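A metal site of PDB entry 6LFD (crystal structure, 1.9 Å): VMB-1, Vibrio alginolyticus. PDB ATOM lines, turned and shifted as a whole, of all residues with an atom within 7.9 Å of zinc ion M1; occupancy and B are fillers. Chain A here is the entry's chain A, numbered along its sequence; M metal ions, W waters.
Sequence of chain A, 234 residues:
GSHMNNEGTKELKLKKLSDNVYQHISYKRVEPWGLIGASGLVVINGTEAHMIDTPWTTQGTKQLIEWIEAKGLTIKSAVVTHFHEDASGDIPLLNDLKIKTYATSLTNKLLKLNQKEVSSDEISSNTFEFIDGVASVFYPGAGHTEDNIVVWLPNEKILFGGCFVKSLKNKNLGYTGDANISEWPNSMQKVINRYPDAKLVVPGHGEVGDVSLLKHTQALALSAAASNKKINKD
A ring nitrogen (NE2) of His 84 lies within hydrogen-bond range of the side-chain carboxylate (OD2) of Asp 178 (2.8 Å).
ND2 of Asn 148 sits close to N of His 144 (2.9 Å).
OD1 of Asp 86 touches zinc ion M1, 3.9 Å away.
Four residues have an atom within 4 Å of zinc ion M1: His 82, His 84, Asp 86 and His 144.
Along chain A the residues within 4 Å of zinc ion M1 span positions 82 to 144.
The nearest printed residue that does not touch zinc ion M1 is Cys 163 (4.1 Å).
Zinc ion M1 is bound by a ring nitrogen (ND1) of His 84.
NE2 of His 144 is bound to zinc ion M1, 2.0 Å away.
NE2 of His 82 is bound to zinc ion M1.
Water W1 binds zinc ion M1, 2.2 Å away.
Zinc ion M1 has four donor atoms within binding distance.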
ATOM      1  N   HIS A  82      10.520  15.121 -11.442  1.00  0.00           N
ATOM      2  CA  HIS A  82      10.832  14.385 -12.684  1.00  0.00           C
ATOM      3  C   HIS A  82      10.352  15.172 -13.901  1.00  0.00           C
ATOM      4  O   HIS A  82       9.676  16.209 -13.733  1.00  0.00           O
ATOM      5  CB  HIS A  82      10.319  12.931 -12.621  1.00  0.00           C
ATOM      6  CG  HIS A  82       8.845  12.755 -12.757  1.00  0.00           C
ATOM      7  ND1 HIS A  82       7.928  13.146 -11.792  1.00  0.00           N
ATOM      8  CD2 HIS A  82       8.142  12.078 -13.696  1.00  0.00           C
ATOM      9  CE1 HIS A  82       6.713  12.736 -12.169  1.00  0.00           C
ATOM     10  NE2 HIS A  82       6.835  12.075 -13.328  1.00  0.00           N
ATOM     11  N   PHE A  83      10.689  14.674 -15.094  1.00  0.00           N
ATOM     12  CA  PHE A  83      10.530  15.428 -16.370  1.00  0.00           C
ATOM     13  C   PHE A  83       9.090  15.395 -16.896  1.00  0.00           C
ATOM     14  O   PHE A  83       8.844  16.142 -17.851  1.00  0.00           O
ATOM     15  CB  PHE A  83      11.533  14.915 -17.401  1.00  0.00           C
ATOM     16  CG  PHE A  83      11.124  13.696 -18.203  1.00  0.00           C
ATOM     17  CD1 PHE A  83      10.456  13.828 -19.405  1.00  0.00           C
ATOM     18  CD2 PHE A  83      11.445  12.423 -17.765  1.00  0.00           C
ATOM     19  CE1 PHE A  83      10.106  12.714 -20.144  1.00  0.00           C
ATOM     20  CE2 PHE A  83      11.106  11.309 -18.518  1.00  0.00           C
ATOM     21  CZ  PHE A  83      10.443  11.454 -19.710  1.00  0.00           C
ATOM     22  N   HIS A  84       8.174  14.590 -16.353  1.00  0.00           N
ATOM     23  CA  HIS A  84       6.758  14.539 -16.845  1.00  0.00           C
ATOM     24  C   HIS A  84       6.023  15.841 -16.495  1.00  0.00           C
ATOM     25  O   HIS A  84       6.431  16.521 -15.549  1.00  0.00           O
ATOM     26  CB  HIS A  84       5.978  13.362 -16.273  1.00  0.00           C
ATOM     27  CG  HIS A  84       6.439  12.024 -16.772  1.00  0.00           C
ATOM     28  ND1 HIS A  84       6.202  10.855 -16.083  1.00  0.00           N
ATOM     29  CD2 HIS A  84       7.129  11.684 -17.885  1.00  0.00           C
ATOM     30  CE1 HIS A  84       6.719   9.852 -16.777  1.00  0.00           C
ATOM     31  NE2 HIS A  84       7.319  10.352 -17.851  1.00  0.00           N
ATOM     32  N   GLU A  85       4.943  16.109 -17.226  1.00  0.00           N
ATOM     33  CA  GLU A  85       4.171  17.396 -17.180  1.00  0.00           C
ATOM     34  C   GLU A  85       3.549  17.628 -15.791  1.00  0.00           C
ATOM     35  O   GLU A  85       3.287  18.813 -15.436  1.00  0.00           O
ATOM     36  CB  GLU A  85       3.067  17.357 -18.249  1.00  0.00           C
ATOM     37  CG  GLU A  85       3.593  17.400 -19.675  1.00  0.00           C
ATOM     38  CD  GLU A  85       3.731  18.778 -20.320  1.00  0.00           C
ATOM     39  OE1 GLU A  85       2.979  19.703 -19.926  1.00  0.00           O
ATOM     40  OE2 GLU A  85       4.585  18.933 -21.231  1.00  0.00           O
ATOM     41  N   ASP A  86       3.299  16.578 -15.017  1.00  0.00           N
ATOM     42  CA  ASP A  86       2.696  16.731 -13.660  1.00  0.00           C
ATOM     43  C   ASP A  86       3.761  17.137 -12.618  1.00  0.00           C
ATOM     44  O   ASP A  86       3.394  17.348 -11.455  1.00  0.00           O
ATOM     45  CB  ASP A  86       1.909  15.496 -13.257  1.00  0.00           C
ATOM     46  CG  ASP A  86       2.721  14.225 -13.252  1.00  0.00           C
ATOM     47  OD1 ASP A  86       3.680  14.122 -14.034  1.00  0.00           O
ATOM     48  OD2 ASP A  86       2.403  13.388 -12.454  1.00  0.00           O
ATOM     49  N   ALA A  87       5.033  17.273 -12.999  1.00  0.00           N
ATOM     50  CA  ALA A  87       6.105  17.754 -12.102  1.00  0.00           C
ATOM     51  C   ALA A  87       6.790  18.978 -12.683  1.00  0.00           C
ATOM     52  O   ALA A  87       7.195  19.863 -11.912  1.00  0.00           O
ATOM     53  CB  ALA A  87       7.103  16.634 -11.860  1.00  0.00           C
ATOM     54  N   HIS A 144      10.107   5.106 -11.507  1.00  0.00           N
ATOM     55  CA  HIS A 144       9.072   5.666 -12.401  1.00  0.00           C
ATOM     56  C   HIS A 144       9.709   6.275 -13.657  1.00  0.00           C
ATOM     57  O   HIS A 144       9.138   6.101 -14.761  1.00  0.00           O
ATOM     58  CB  HIS A 144       8.205   6.655 -11.612  1.00  0.00           C
ATOM     59  CG  HIS A 144       7.270   7.425 -12.471  1.00  0.00           C
ATOM     60  ND1 HIS A 144       6.209   6.828 -13.127  1.00  0.00           N
ATOM     61  CD2 HIS A 144       7.236   8.740 -12.785  1.00  0.00           C
ATOM     62  CE1 HIS A 144       5.549   7.754 -13.798  1.00  0.00           C
ATOM     63  NE2 HIS A 144       6.141   8.928 -13.590  1.00  0.00           N
ATOM     64  N   THR A 145      10.823   6.989 -13.512  1.00  0.00           N
ATOM     65  CA  THR A 145      11.645   7.516 -14.620  1.00  0.00           C
ATOM     66  C   THR A 145      13.114   7.364 -14.231  1.00  0.00           C
ATOM     67  O   THR A 145      13.393   7.049 -13.068  1.00  0.00           O
ATOM     68  CB  THR A 145      11.297   8.974 -14.965  1.00  0.00           C
ATOM     69  OG1 THR A 145      11.533   9.780 -13.802  1.00  0.00           O
ATOM     70  CG2 THR A 145       9.891   9.151 -15.498  1.00  0.00           C
ATOM     71  N   ASP A 147      15.125   9.803 -13.935  1.00  0.00           N
ATOM     72  CA  ASP A 147      15.524  11.078 -13.305  1.00  0.00           C
ATOM     73  C   ASP A 147      14.799  11.337 -11.966  1.00  0.00           C
ATOM     74  O   ASP A 147      15.145  12.319 -11.318  1.00  0.00           O
ATOM     75  CB  ASP A 147      15.261  12.253 -14.260  1.00  0.00           C
ATOM     76  CG  ASP A 147      13.792  12.433 -14.616  1.00  0.00           C
ATOM     77  OD1 ASP A 147      13.112  11.426 -14.871  1.00  0.00           O
ATOM     78  OD2 ASP A 147      13.340  13.586 -14.645  1.00  0.00           O
ATOM     79  N   ASN A 148      13.877  10.493 -11.529  1.00  0.00           N
ATOM     80  CA  ASN A 148      12.960  10.851 -10.408  1.00  0.00           C
ATOM     81  C   ASN A 148      13.766  11.115  -9.129  1.00  0.00           C
ATOM     82  O   ASN A 148      14.710  10.355  -8.838  1.00  0.00           O
ATOM     83  CB  ASN A 148      11.862   9.811 -10.160  1.00  0.00           C
ATOM     84  CG  ASN A 148      12.350   8.383 -10.118  1.00  0.00           C
ATOM     85  OD1 ASN A 148      13.497   8.088  -9.733  1.00  0.00           O
ATOM     86  ND2 ASN A 148      11.463   7.488 -10.501  1.00  0.00           N
ATOM     87  N   GLY A 162       6.858  11.853  -4.748  1.00  0.00           N
ATOM     88  CA  GLY A 162       6.353  12.092  -6.108  1.00  0.00           C
ATOM     89  C   GLY A 162       5.929  10.786  -6.785  1.00  0.00           C
ATOM     90  O   GLY A 162       5.558   9.852  -6.102  1.00  0.00           O
ATOM     91  N   CYS A 163       6.055  10.705  -8.096  1.00  0.00           N
ATOM     92  CA  CYS A 163       5.532   9.562  -8.879  1.00  0.00           C
ATOM     93  C   CYS A 163       6.467   8.353  -8.761  1.00  0.00           C
ATOM     94  O   CYS A 163       6.083   7.242  -9.207  1.00  0.00           O
ATOM     95  CB  CYS A 163       5.228  10.023 -10.286  1.00  0.00           C
ATOM     96  SG  CYS A 163       4.163  11.483 -10.233  1.00  0.00           S
ATOM     97  N   PHE A 164       7.615   8.520  -8.095  1.00  0.00           N
ATOM     98  CA  PHE A 164       8.480   7.400  -7.635  1.00  0.00           C
ATOM     99  C   PHE A 164       7.751   6.523  -6.589  1.00  0.00           C
ATOM    100  O   PHE A 164       8.093   5.313  -6.394  1.00  0.00           O
ATOM    101  CB  PHE A 164       9.778   7.988  -7.073  1.00  0.00           C
ATOM    102  CG  PHE A 164      10.778   6.967  -6.595  1.00  0.00           C
ATOM    103  CD1 PHE A 164      11.471   6.179  -7.507  1.00  0.00           C
ATOM    104  CD2 PHE A 164      11.049   6.825  -5.252  1.00  0.00           C
ATOM    105  CE1 PHE A 164      12.413   5.258  -7.079  1.00  0.00           C
ATOM    106  CE2 PHE A 164      11.976   5.892  -4.820  1.00  0.00           C
ATOM    107  CZ  PHE A 164      12.669   5.132  -5.741  1.00  0.00           C
ATOM    108  N   TYR A 175       1.829   4.569 -15.442  1.00  0.00           N
ATOM    109  CA  TYR A 175       2.516   4.711 -16.743  1.00  0.00           C
ATOM    110  C   TYR A 175       3.977   4.303 -16.556  1.00  0.00           C
ATOM    111  O   TYR A 175       4.639   4.960 -15.742  1.00  0.00           O
ATOM    112  CB  TYR A 175       2.371   6.124 -17.279  1.00  0.00           C
ATOM    113  CG  TYR A 175       3.183   6.357 -18.518  1.00  0.00           C
ATOM    114  CD1 TYR A 175       2.773   5.863 -19.745  1.00  0.00           C
ATOM    115  CD2 TYR A 175       4.384   7.035 -18.465  1.00  0.00           C
ATOM    116  CE1 TYR A 175       3.507   6.060 -20.889  1.00  0.00           C
ATOM    117  CE2 TYR A 175       5.134   7.258 -19.613  1.00  0.00           C
ATOM    118  CZ  TYR A 175       4.697   6.767 -20.830  1.00  0.00           C
ATOM    119  OH  TYR A 175       5.436   6.948 -21.956  1.00  0.00           O
ATOM    120  N   ASP A 178       8.397   5.206 -19.349  1.00  0.00           N
ATOM    121  CA  ASP A 178       9.732   5.783 -19.049  1.00  0.00           C
ATOM    122  C   ASP A 178      10.373   5.120 -17.832  1.00  0.00           C
ATOM    123  O   ASP A 178      11.399   5.634 -17.379  1.00  0.00           O
ATOM    124  CB  ASP A 178       9.590   7.295 -18.867  1.00  0.00           C
ATOM    125  CG  ASP A 178       9.107   7.977 -20.132  1.00  0.00           C
ATOM    126  OD1 ASP A 178       9.489   7.505 -21.212  1.00  0.00           O
ATOM    127  OD2 ASP A 178       8.341   8.941 -20.035  1.00  0.00           O
ATOM    128  N   HIS A 205       0.449  10.871  -6.894  1.00  0.00           N
ATOM    129  CA  HIS A 205      -1.022  10.682  -7.064  1.00  0.00           C
ATOM    130  C   HIS A 205      -1.553   9.801  -5.932  1.00  0.00           C
ATOM    131  O   HIS A 205      -0.866   8.797  -5.578  1.00  0.00           O
ATOM    132  CB  HIS A 205      -1.349  10.019  -8.421  1.00  0.00           C
ATOM    133  CG  HIS A 205      -0.582  10.568  -9.574  1.00  0.00           C
ATOM    134  ND1 HIS A 205      -1.022  11.677 -10.290  1.00  0.00           N
ATOM    135  CD2 HIS A 205       0.575  10.181 -10.152  1.00  0.00           C
ATOM    136  CE1 HIS A 205      -0.171  11.927 -11.268  1.00  0.00           C
ATOM    137  NE2 HIS A 205       0.831  11.038 -11.181  1.00  0.00           N
HETATM  138 ZN    ZN M   1       5.547  10.709 -14.300  1.00  0.00          ZN
HETATM  139 ZN    ZN M   2       2.731  11.462 -12.070  1.00  0.00          ZN
HETATM  140  O   HOH W   1       3.385  10.622 -13.948  1.00  0.00           O
